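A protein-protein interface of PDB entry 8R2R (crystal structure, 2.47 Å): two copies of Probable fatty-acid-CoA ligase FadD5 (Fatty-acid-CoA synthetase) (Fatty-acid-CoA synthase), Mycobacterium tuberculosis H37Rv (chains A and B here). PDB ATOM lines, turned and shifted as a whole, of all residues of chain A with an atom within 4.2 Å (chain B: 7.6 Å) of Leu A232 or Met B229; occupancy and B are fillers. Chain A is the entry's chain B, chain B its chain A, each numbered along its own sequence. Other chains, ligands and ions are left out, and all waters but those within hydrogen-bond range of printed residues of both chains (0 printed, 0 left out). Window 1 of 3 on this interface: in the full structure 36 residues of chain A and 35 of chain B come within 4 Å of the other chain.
The side-chain hydroxyl (OG1) of Thr B378 sits at hydrogen-bond distance from the side-chain hydroxyl (OH) of Tyr B233 (2.7 Å). The side-chain hydroxyl (OG1) of Thr A230 is in hydrogen-bond range of the side-chain hydroxyl (OH) of Tyr A233 (3.4 Å).
Hydrophobic or aromatic side chains of chain A within 4 Å of the printed part of chain B: Met A229, Leu A232, Tyr A233, Leu A264 and Leu A265. Printed residues of chain B that touch a printed residue of chain A: Met B229, Leu B232, Tyr B233, Ala B237, Leu B265 and Thr B378. Among the printed residues, 10 pairs touch across the chains.
Met B229 touches its own counterpart, Met A229. Met A229 touches Leu B232, and with the chains exchanged Leu A232 touches Met B229. Leu A232 touches Tyr B233, and with the chains exchanged Tyr A233 touches Leu B232. Tyr A233 touches Leu B265, and with the chains exchanged Leu A265 touches Tyr B233. Positions printed for both chains: 228, 229, 230, 231, 232, 233, 234, 236, 264 and 265. Of the 10 pairs that touch across the chains among the printed residues, 8 have their exchanged pair printed and touching as well.
Of chain B, only Met B229 (3.6 Å), Leu B232 (3.9 Å) and Tyr B233 (3.8 Å) come within 4 Å of Leu A232. Printed residues of chain A within 4 Å of Met B229: Met A229 (3.5 Å) and Leu A232 (3.6 Å). Printed residues of chain B within 4 Å of Met A229: Met B229 (3.5 Å) and Leu B232 (3.7 Å). Of the printed residues of chain A, Ala B237 touches Tyr A233. Of the printed residues of chain A, Leu B232 touches Met A229, Leu A232 and Tyr A233. Of the printed residues of chain A, Leu B265 touches Tyr A233 (3.5 Å). The nearest printed residue of chain B that does not touch Tyr A233 is Asn B238 (5.1 Å).
The backbone carbonyl oxygen (O) of Tyr A233 sits close to the backbone carbonyl oxygen (O) of Ala B237, 3.4 Å away.
Among the printed residues, pairs that only touch across the chains: Leu A265 with Tyr B233 (3.5 Å), Tyr A233 with Leu B265 (3.5 Å), Met A229 with Met B229 (3.5 Å), Leu A232 with Met B229 (3.6 Å), Met A229 with Leu B232 (3.7 Å), Leu A232 with Tyr B233 (3.8 Å), Leu A232 with Leu B232 (3.9 Å), Tyr A233 with Leu B232 (3.9 Å) and Leu A264 with Thr B378 (3.9 Å).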
ATOM      1  N   GLN A  42     -16.265 -34.889  10.857  1.00  0.00           N
ATOM      2  CA  GLN A  42     -16.949 -34.109   9.828  1.00  0.00           C
ATOM      3  C   GLN A  42     -17.720 -35.065   8.923  1.00  0.00           C
ATOM      4  O   GLN A  42     -17.118 -35.842   8.174  1.00  0.00           O
ATOM      5  CB  GLN A  42     -15.960 -33.257   9.026  1.00  0.00           C
ATOM      6  CG  GLN A  42     -16.603 -32.381   7.938  1.00  0.00           C
ATOM      7  CD  GLN A  42     -17.561 -31.331   8.491  1.00  0.00           C
ATOM      8  OE1 GLN A  42     -18.683 -31.643   8.891  1.00  0.00           O
ATOM      9  NE2 GLN A  42     -17.121 -30.076   8.503  1.00  0.00           N
ATOM     10  N   ALA A 228     -17.906 -31.841  -1.605  1.00  0.00           N
ATOM     11  CA  ALA A 228     -18.567 -30.583  -1.265  1.00  0.00           C
ATOM     12  C   ALA A 228     -17.607 -29.418  -1.419  1.00  0.00           C
ATOM     13  O   ALA A 228     -18.003 -28.330  -1.851  1.00  0.00           O
ATOM     14  CB  ALA A 228     -19.123 -30.622   0.161  1.00  0.00           C
ATOM     15  N   MET A 229     -16.337 -29.634  -1.078  1.00  0.00           N
ATOM     16  CA  MET A 229     -15.335 -28.587  -1.239  1.00  0.00           C
ATOM     17  C   MET A 229     -15.249 -28.131  -2.689  1.00  0.00           C
ATOM     18  O   MET A 229     -15.224 -26.927  -2.970  1.00  0.00           O
ATOM     19  CB  MET A 229     -13.982 -29.094  -0.746  1.00  0.00           C
ATOM     20  CG  MET A 229     -13.064 -28.002  -0.255  1.00  0.00           C
ATOM     21  SD  MET A 229     -11.684 -28.684   0.676  1.00  0.00           S
ATOM     22  CE  MET A 229     -12.550 -29.494   2.024  1.00  0.00           C
ATOM     23  N   THR A 230     -15.231 -29.085  -3.625  1.00  0.00           N
ATOM     24  CA  THR A 230     -15.185 -28.748  -5.045  1.00  0.00           C
ATOM     25  C   THR A 230     -16.361 -27.863  -5.448  1.00  0.00           C
ATOM     26  O   THR A 230     -16.212 -26.957  -6.277  1.00  0.00           O
ATOM     27  CB  THR A 230     -15.160 -30.030  -5.875  1.00  0.00           C
ATOM     28  OG1 THR A 230     -13.940 -30.735  -5.616  1.00  0.00           O
ATOM     29  CG2 THR A 230     -15.257 -29.717  -7.358  1.00  0.00           C
ATOM     30  N   ALA A 231     -17.534 -28.094  -4.862  1.00  0.00           N
ATOM     31  CA  ALA A 231     -18.668 -27.230  -5.161  1.00  0.00           C
ATOM     32  C   ALA A 231     -18.479 -25.839  -4.569  1.00  0.00           C
ATOM     33  O   ALA A 231     -18.975 -24.856  -5.130  1.00  0.00           O
ATOM     34  CB  ALA A 231     -19.962 -27.864  -4.650  1.00  0.00           C
ATOM     35  N   LEU A 232     -17.744 -25.732  -3.459  1.00  0.00           N
ATOM     36  CA  LEU A 232     -17.575 -24.437  -2.802  1.00  0.00           C
ATOM     37  C   LEU A 232     -16.657 -23.508  -3.588  1.00  0.00           C
ATOM     38  O   LEU A 232     -16.915 -22.301  -3.663  1.00  0.00           O
ATOM     39  CB  LEU A 232     -17.038 -24.632  -1.386  1.00  0.00           C
ATOM     40  CG  LEU A 232     -18.001 -25.292  -0.408  1.00  0.00           C
ATOM     41  CD1 LEU A 232     -17.361 -25.373   0.965  1.00  0.00           C
ATOM     42  CD2 LEU A 232     -19.316 -24.520  -0.359  1.00  0.00           C
ATOM     43  N   TYR A 233     -15.576 -24.034  -4.164  1.00  0.00           N
ATOM     44  CA  TYR A 233     -14.623 -23.188  -4.870  1.00  0.00           C
ATOM     45  C   TYR A 233     -14.878 -23.122  -6.369  1.00  0.00           C
ATOM     46  O   TYR A 233     -14.026 -22.629  -7.112  1.00  0.00           O
ATOM     47  CB  TYR A 233     -13.179 -23.626  -4.589  1.00  0.00           C
ATOM     48  CG  TYR A 233     -12.730 -24.990  -5.076  1.00  0.00           C
ATOM     49  CD1 TYR A 233     -12.540 -25.253  -6.429  1.00  0.00           C
ATOM     50  CD2 TYR A 233     -12.404 -25.989  -4.166  1.00  0.00           C
ATOM     51  CE1 TYR A 233     -12.090 -26.491  -6.862  1.00  0.00           C
ATOM     52  CE2 TYR A 233     -11.952 -27.224  -4.589  1.00  0.00           C
ATOM     53  CZ  TYR A 233     -11.799 -27.472  -5.934  1.00  0.00           C
ATOM     54  OH  TYR A 233     -11.348 -28.707  -6.347  1.00  0.00           O
ATOM     55  N   THR A 234     -16.031 -23.593  -6.827  1.00  0.00           N
ATOM     56  CA  THR A 234     -16.461 -23.394  -8.205  1.00  0.00           C
ATOM     57  C   THR A 234     -17.769 -22.626  -8.286  1.00  0.00           C
ATOM     58  O   THR A 234     -17.845 -21.613  -8.988  1.00  0.00           O
ATOM     59  CB  THR A 234     -16.599 -24.747  -8.919  1.00  0.00           C
ATOM     60  OG1 THR A 234     -17.487 -25.587  -8.173  1.00  0.00           O
ATOM     61  CG2 THR A 234     -15.241 -25.432  -9.031  1.00  0.00           C
ATOM     62  N   GLY A 236     -19.313 -21.275  -5.496  1.00  0.00           N
ATOM     63  CA  GLY A 236     -19.403 -20.286  -4.445  1.00  0.00           C
ATOM     64  C   GLY A 236     -20.590 -20.557  -3.540  1.00  0.00           C
ATOM     65  O   GLY A 236     -21.259 -21.594  -3.633  1.00  0.00           O
ATOM     66  N   LEU A 264     -24.073 -29.215   4.364  1.00  0.00           N
ATOM     67  CA  LEU A 264     -22.877 -28.656   4.988  1.00  0.00           C
ATOM     68  C   LEU A 264     -23.137 -27.249   5.506  1.00  0.00           C
ATOM     69  O   LEU A 264     -22.870 -26.946   6.676  1.00  0.00           O
ATOM     70  CB  LEU A 264     -21.713 -28.654   3.996  1.00  0.00           C
ATOM     71  CG  LEU A 264     -20.404 -28.020   4.468  1.00  0.00           C
ATOM     72  CD1 LEU A 264     -19.816 -28.814   5.611  1.00  0.00           C
ATOM     73  CD2 LEU A 264     -19.427 -27.932   3.314  1.00  0.00           C
ATOM     74  N   LEU A 265     -23.673 -26.380   4.653  1.00  0.00           N
ATOM     75  CA  LEU A 265     -23.813 -24.966   4.965  1.00  0.00           C
ATOM     76  C   LEU A 265     -25.111 -24.633   5.689  1.00  0.00           C
ATOM     77  O   LEU A 265     -25.320 -23.465   6.038  1.00  0.00           O
ATOM     78  CB  LEU A 265     -23.706 -24.137   3.681  1.00  0.00           C
ATOM     79  CG  LEU A 265     -22.396 -24.300   2.895  1.00  0.00           C
ATOM     80  CD1 LEU A 265     -22.410 -23.440   1.652  1.00  0.00           C
ATOM     81  CD2 LEU A 265     -21.187 -23.963   3.758  1.00  0.00           C
ATOM     82  N   ASN B 223      -7.210 -29.705  10.725  1.00  0.00           N
ATOM     83  CA  ASN B 223      -7.578 -28.382  11.220  1.00  0.00           C
ATOM     84  C   ASN B 223      -7.436 -27.334  10.124  1.00  0.00           C
ATOM     85  O   ASN B 223      -8.377 -26.584   9.839  1.00  0.00           O
ATOM     86  CB  ASN B 223      -6.706 -28.035  12.430  1.00  0.00           C
ATOM     87  CG  ASN B 223      -7.156 -26.780  13.145  1.00  0.00           C
ATOM     88  OD1 ASN B 223      -7.431 -25.751  12.527  1.00  0.00           O
ATOM     89  ND2 ASN B 223      -7.227 -26.859  14.467  1.00  0.00           N
ATOM     90  N   LEU B 224      -6.265 -27.285   9.481  1.00  0.00           N
ATOM     91  CA  LEU B 224      -6.017 -26.284   8.446  1.00  0.00           C
ATOM     92  C   LEU B 224      -6.943 -26.468   7.251  1.00  0.00           C
ATOM     93  O   LEU B 224      -7.464 -25.485   6.706  1.00  0.00           O
ATOM     94  CB  LEU B 224      -4.560 -26.344   7.998  1.00  0.00           C
ATOM     95  CG  LEU B 224      -3.550 -25.992   9.084  1.00  0.00           C
ATOM     96  CD1 LEU B 224      -2.146 -26.228   8.588  1.00  0.00           C
ATOM     97  CD2 LEU B 224      -3.738 -24.551   9.505  1.00  0.00           C
ATOM     98  N   THR B 225      -7.144 -27.720   6.817  1.00  0.00           N
ATOM     99  CA  THR B 225      -8.081 -27.986   5.728  1.00  0.00           C
ATOM    100  C   THR B 225      -9.453 -27.404   6.032  1.00  0.00           C
ATOM    101  O   THR B 225     -10.035 -26.696   5.202  1.00  0.00           O
ATOM    102  CB  THR B 225      -8.216 -29.486   5.477  1.00  0.00           C
ATOM    103  OG1 THR B 225      -6.927 -30.065   5.236  1.00  0.00           O
ATOM    104  CG2 THR B 225      -9.115 -29.708   4.273  1.00  0.00           C
ATOM    105  N   GLY B 226      -9.982 -27.689   7.221  1.00  0.00           N
ATOM    106  CA  GLY B 226     -11.285 -27.165   7.576  1.00  0.00           C
ATOM    107  C   GLY B 226     -11.321 -25.650   7.589  1.00  0.00           C
ATOM    108  O   GLY B 226     -12.325 -25.045   7.198  1.00  0.00           O
ATOM    109  N   GLN B 227     -10.234 -25.015   8.042  1.00  0.00           N
ATOM    110  CA  GLN B 227     -10.196 -23.557   8.038  1.00  0.00           C
ATOM    111  C   GLN B 227     -10.160 -23.014   6.619  1.00  0.00           C
ATOM    112  O   GLN B 227     -10.701 -21.932   6.361  1.00  0.00           O
ATOM    113  CB  GLN B 227      -8.997 -23.040   8.843  1.00  0.00           C
ATOM    114  CG  GLN B 227      -9.047 -23.434  10.318  1.00  0.00           C
ATOM    115  CD  GLN B 227      -8.414 -22.414  11.236  1.00  0.00           C
ATOM    116  OE1 GLN B 227      -8.679 -21.211  11.136  1.00  0.00           O
ATOM    117  NE2 GLN B 227      -7.570 -22.890  12.144  1.00  0.00           N
ATOM    118  N   ALA B 228      -9.535 -23.749   5.693  1.00  0.00           N
ATOM    119  CA  ALA B 228      -9.555 -23.342   4.292  1.00  0.00           C
ATOM    120  C   ALA B 228     -10.967 -23.375   3.731  1.00  0.00           C
ATOM    121  O   ALA B 228     -11.329 -22.524   2.908  1.00  0.00           O
ATOM    122  CB  ALA B 228      -8.638 -24.241   3.461  1.00  0.00           C
ATOM    123  N   MET B 229     -11.774 -24.340   4.178  1.00  0.00           N
ATOM    124  CA  MET B 229     -13.143 -24.461   3.695  1.00  0.00           C
ATOM    125  C   MET B 229     -13.980 -23.251   4.083  1.00  0.00           C
ATOM    126  O   MET B 229     -14.838 -22.816   3.304  1.00  0.00           O
ATOM    127  CB  MET B 229     -13.759 -25.752   4.232  1.00  0.00           C
ATOM    128  CG  MET B 229     -14.759 -26.402   3.300  1.00  0.00           C
ATOM    129  SD  MET B 229     -15.174 -28.071   3.830  1.00  0.00           S
ATOM    130  CE  MET B 229     -15.762 -27.782   5.502  1.00  0.00           C
ATOM    131  N   THR B 230     -13.736 -22.682   5.269  1.00  0.00           N
ATOM    132  CA  THR B 230     -14.484 -21.499   5.685  1.00  0.00           C
ATOM    133  C   THR B 230     -14.221 -20.325   4.755  1.00  0.00           C
ATOM    134  O   THR B 230     -15.118 -19.515   4.491  1.00  0.00           O
ATOM    135  CB  THR B 230     -14.128 -21.123   7.121  1.00  0.00           C
ATOM    136  OG1 THR B 230     -14.436 -22.214   7.993  1.00  0.00           O
ATOM    137  CG2 THR B 230     -14.914 -19.887   7.562  1.00  0.00           C
ATOM    138  N   ALA B 231     -12.992 -20.210   4.252  1.00  0.00           N
ATOM    139  CA  ALA B 231     -12.705 -19.145   3.301  1.00  0.00           C
ATOM    140  C   ALA B 231     -13.460 -19.349   2.000  1.00  0.00           C
ATOM    141  O   ALA B 231     -13.881 -18.373   1.369  1.00  0.00           O
ATOM    142  CB  ALA B 231     -11.205 -19.061   3.041  1.00  0.00           C
ATOM    143  N   LEU B 232     -13.659 -20.606   1.599  1.00  0.00           N
ATOM    144  CA  LEU B 232     -14.286 -20.884   0.310  1.00  0.00           C
ATOM    145  C   LEU B 232     -15.759 -20.501   0.306  1.00  0.00           C
ATOM    146  O   LEU B 232     -16.256 -19.938  -0.677  1.00  0.00           O
ATOM    147  CB  LEU B 232     -14.123 -22.358  -0.039  1.00  0.00           C
ATOM    148  CG  LEU B 232     -12.680 -22.822  -0.157  1.00  0.00           C
ATOM    149  CD1 LEU B 232     -12.649 -24.322  -0.412  1.00  0.00           C
ATOM    150  CD2 LEU B 232     -11.954 -22.057  -1.270  1.00  0.00           C
ATOM    151  N   TYR B 233     -16.478 -20.799   1.383  1.00  0.00           N
ATOM    152  CA  TYR B 233     -17.916 -20.582   1.363  1.00  0.00           C
ATOM    153  C   TYR B 233     -18.317 -19.216   1.899  1.00  0.00           C
ATOM    154  O   TYR B 233     -19.513 -18.904   1.932  1.00  0.00           O
ATOM    155  CB  TYR B 233     -18.648 -21.713   2.108  1.00  0.00           C
ATOM    156  CG  TYR B 233     -18.439 -21.867   3.605  1.00  0.00           C
ATOM    157  CD1 TYR B 233     -18.898 -20.904   4.501  1.00  0.00           C
ATOM    158  CD2 TYR B 233     -17.870 -23.028   4.128  1.00  0.00           C
ATOM    159  CE1 TYR B 233     -18.747 -21.064   5.864  1.00  0.00           C
ATOM    160  CE2 TYR B 233     -17.714 -23.199   5.493  1.00  0.00           C
ATOM    161  CZ  TYR B 233     -18.157 -22.211   6.358  1.00  0.00           C
ATOM    162  OH  TYR B 233     -18.013 -22.363   7.722  1.00  0.00           O
ATOM    163  N   THR B 234     -17.352 -18.386   2.287  1.00  0.00           N
ATOM    164  CA  THR B 234     -17.607 -16.988   2.607  1.00  0.00           C
ATOM    165  C   THR B 234     -17.084 -16.048   1.533  1.00  0.00           C
ATOM    166  O   THR B 234     -17.848 -15.244   0.989  1.00  0.00           O
ATOM    167  CB  THR B 234     -16.980 -16.631   3.963  1.00  0.00           C
ATOM    168  OG1 THR B 234     -15.576 -16.900   3.921  1.00  0.00           O
ATOM    169  CG2 THR B 234     -17.605 -17.457   5.072  1.00  0.00           C
ATOM    170  N   SER B 235     -15.790 -16.135   1.203  1.00  0.00           N
ATOM    171  CA  SER B 235     -15.192 -15.258   0.202  1.00  0.00           C
ATOM    172  C   SER B 235     -15.487 -15.701  -1.219  1.00  0.00           C
ATOM    173  O   SER B 235     -15.498 -14.859  -2.124  1.00  0.00           O
ATOM    174  CB  SER B 235     -13.669 -15.186   0.368  1.00  0.00           C
ATOM    175  OG  SER B 235     -13.287 -14.821   1.681  1.00  0.00           O
ATOM    176  N   GLY B 236     -15.720 -16.991  -1.437  1.00  0.00           N
ATOM    177  CA  GLY B 236     -15.757 -17.524  -2.780  1.00  0.00           C
ATOM    178  C   GLY B 236     -14.355 -17.694  -3.340  1.00  0.00           C
ATOM    179  O   GLY B 236     -13.341 -17.482  -2.669  1.00  0.00           O
ATOM    180  N   ALA B 237     -14.306 -18.077  -4.616  1.00  0.00           N
ATOM    181  CA  ALA B 237     -13.042 -18.354  -5.287  1.00  0.00           C
ATOM    182  C   ALA B 237     -13.239 -18.509  -6.784  1.00  0.00           C
ATOM    183  O   ALA B 237     -14.121 -19.258  -7.221  1.00  0.00           O
ATOM    184  CB  ALA B 237     -12.401 -19.632  -4.736  1.00  0.00           C
ATOM    185  N   ASN B 238     -12.419 -17.820  -7.576  1.00  0.00           N
ATOM    186  CA  ASN B 238     -12.315 -18.054  -9.013  1.00  0.00           C
ATOM    187  C   ASN B 238     -10.989 -18.758  -9.271  1.00  0.00           C
ATOM    188  O   ASN B 238      -9.930 -18.132  -9.223  1.00  0.00           O
ATOM    189  CB  ASN B 238     -12.407 -16.753  -9.804  1.00  0.00           C
ATOM    190  CG  ASN B 238     -12.492 -16.987 -11.304  1.00  0.00           C
ATOM    191  OD1 ASN B 238     -11.734 -17.779 -11.878  1.00  0.00           O
ATOM    192  ND2 ASN B 238     -13.424 -16.304 -11.944  1.00  0.00           N
ATOM    193  N   LEU B 260      -3.761 -20.396   2.952  1.00  0.00           N
ATOM    194  CA  LEU B 260      -4.465 -21.665   2.784  1.00  0.00           C
ATOM    195  C   LEU B 260      -5.117 -21.761   1.416  1.00  0.00           C
ATOM    196  O   LEU B 260      -4.984 -22.774   0.721  1.00  0.00           O
ATOM    197  CB  LEU B 260      -5.516 -21.827   3.879  1.00  0.00           C
ATOM    198  CG  LEU B 260      -4.973 -21.869   5.302  1.00  0.00           C
ATOM    199  CD1 LEU B 260      -6.110 -22.005   6.285  1.00  0.00           C
ATOM    200  CD2 LEU B 260      -3.999 -23.018   5.448  1.00  0.00           C
ATOM    201  N   THR B 261      -5.822 -20.704   1.012  1.00  0.00           N
ATOM    202  CA  THR B 261      -6.551 -20.724  -0.251  1.00  0.00           C
ATOM    203  C   THR B 261      -5.613 -20.865  -1.447  1.00  0.00           C
ATOM    204  O   THR B 261      -5.884 -21.643  -2.372  1.00  0.00           O
ATOM    205  CB  THR B 261      -7.396 -19.458  -0.358  1.00  0.00           C
ATOM    206  OG1 THR B 261      -8.643 -19.679   0.311  1.00  0.00           O
ATOM    207  CG2 THR B 261      -7.647 -19.088  -1.798  1.00  0.00           C
ATOM    208  N   LEU B 264      -4.148 -24.452  -1.503  1.00  0.00           N
ATOM    209  CA  LEU B 264      -5.172 -25.446  -1.809  1.00  0.00           C
ATOM    210  C   LEU B 264      -5.577 -25.384  -3.276  1.00  0.00           C
ATOM    211  O   LEU B 264      -5.557 -26.401  -3.982  1.00  0.00           O
ATOM    212  CB  LEU B 264      -6.394 -25.249  -0.907  1.00  0.00           C
ATOM    213  CG  LEU B 264      -7.518 -26.267  -1.150  1.00  0.00           C
ATOM    214  CD1 LEU B 264      -7.008 -27.690  -0.927  1.00  0.00           C
ATOM    215  CD2 LEU B 264      -8.727 -25.987  -0.273  1.00  0.00           C
ATOM    216  N   LEU B 265      -5.937 -24.196  -3.756  1.00  0.00           N
ATOM    217  CA  LEU B 265      -6.484 -24.034  -5.095  1.00  0.00           C
ATOM    218  C   LEU B 265      -5.418 -23.818  -6.158  1.00  0.00           C
ATOM    219  O   LEU B 265      -5.765 -23.655  -7.332  1.00  0.00           O
ATOM    220  CB  LEU B 265      -7.466 -22.863  -5.116  1.00  0.00           C
ATOM    221  CG  LEU B 265      -8.627 -22.943  -4.130  1.00  0.00           C
ATOM    222  CD1 LEU B 265      -9.521 -21.737  -4.317  1.00  0.00           C
ATOM    223  CD2 LEU B 265      -9.409 -24.231  -4.339  1.00  0.00           C
ATOM    224  N   ILE B 376     -20.695 -19.469  11.965  1.00  0.00           N
ATOM    225  CA  ILE B 376     -20.578 -20.067  10.637  1.00  0.00           C
ATOM    226  C   ILE B 376     -21.141 -21.488  10.647  1.00  0.00           C
ATOM    227  O   ILE B 376     -21.178 -22.129  11.708  1.00  0.00           O
ATOM    228  CB  ILE B 376     -19.120 -20.049  10.150  1.00  0.00           C
ATOM    229  CG1 ILE B 376     -18.206 -20.763  11.150  1.00  0.00           C
ATOM    230  CG2 ILE B 376     -18.669 -18.618   9.874  1.00  0.00           C
ATOM    231  CD1 ILE B 376     -16.808 -21.026  10.593  1.00  0.00           C
ATOM    232  N   THR B 378     -20.102 -24.416   9.941  1.00  0.00           N
ATOM    233  CA  THR B 378     -19.253 -25.534  10.333  1.00  0.00           C
ATOM    234  C   THR B 378     -18.764 -25.418  11.774  1.00  0.00           C
ATOM    235  O   THR B 378     -17.780 -26.069  12.141  1.00  0.00           O
ATOM    236  CB  THR B 378     -18.072 -25.658   9.371  1.00  0.00           C
ATOM    237  OG1 THR B 378     -17.342 -24.425   9.340  1.00  0.00           O
ATOM    238  CG2 THR B 378     -18.567 -25.974   7.964  1.00  0.00           C
ATOM    239  N   PRO B 404     -14.715 -29.211  14.353  1.00  0.00           N
ATOM    240  CA  PRO B 404     -13.518 -29.975  13.961  1.00  0.00           C
ATOM    241  C   PRO B 404     -12.282 -29.103  13.792  1.00  0.00           C
ATOM    242  O   PRO B 404     -11.158 -29.590  13.966  1.00  0.00           O
ATOM    243  CB  PRO B 404     -13.929 -30.625  12.629  1.00  0.00           C
ATOM    244  CG  PRO B 404     -15.428 -30.453  12.533  1.00  0.00           C
ATOM    245  CD  PRO B 404     -15.740 -29.208  13.296  1.00  0.00           C
ATOM    246  N   THR B 405     -12.453 -27.823  13.476  1.00  0.00           N
ATOM    247  CA  THR B 405     -11.338 -26.922  13.244  1.00  0.00           C
ATOM    248  C   THR B 405     -10.816 -26.269  14.521  1.00  0.00           C
ATOM    249  O   THR B 405     -10.072 -25.290  14.437  1.00  0.00           O
ATOM    250  CB  THR B 405     -11.739 -25.852  12.227  1.00  0.00           C
ATOM    251  OG1 THR B 405     -12.963 -25.233  12.636  1.00  0.00           O
ATOM    252  CG2 THR B 405     -11.957 -26.491  10.883  1.00  0.00           C
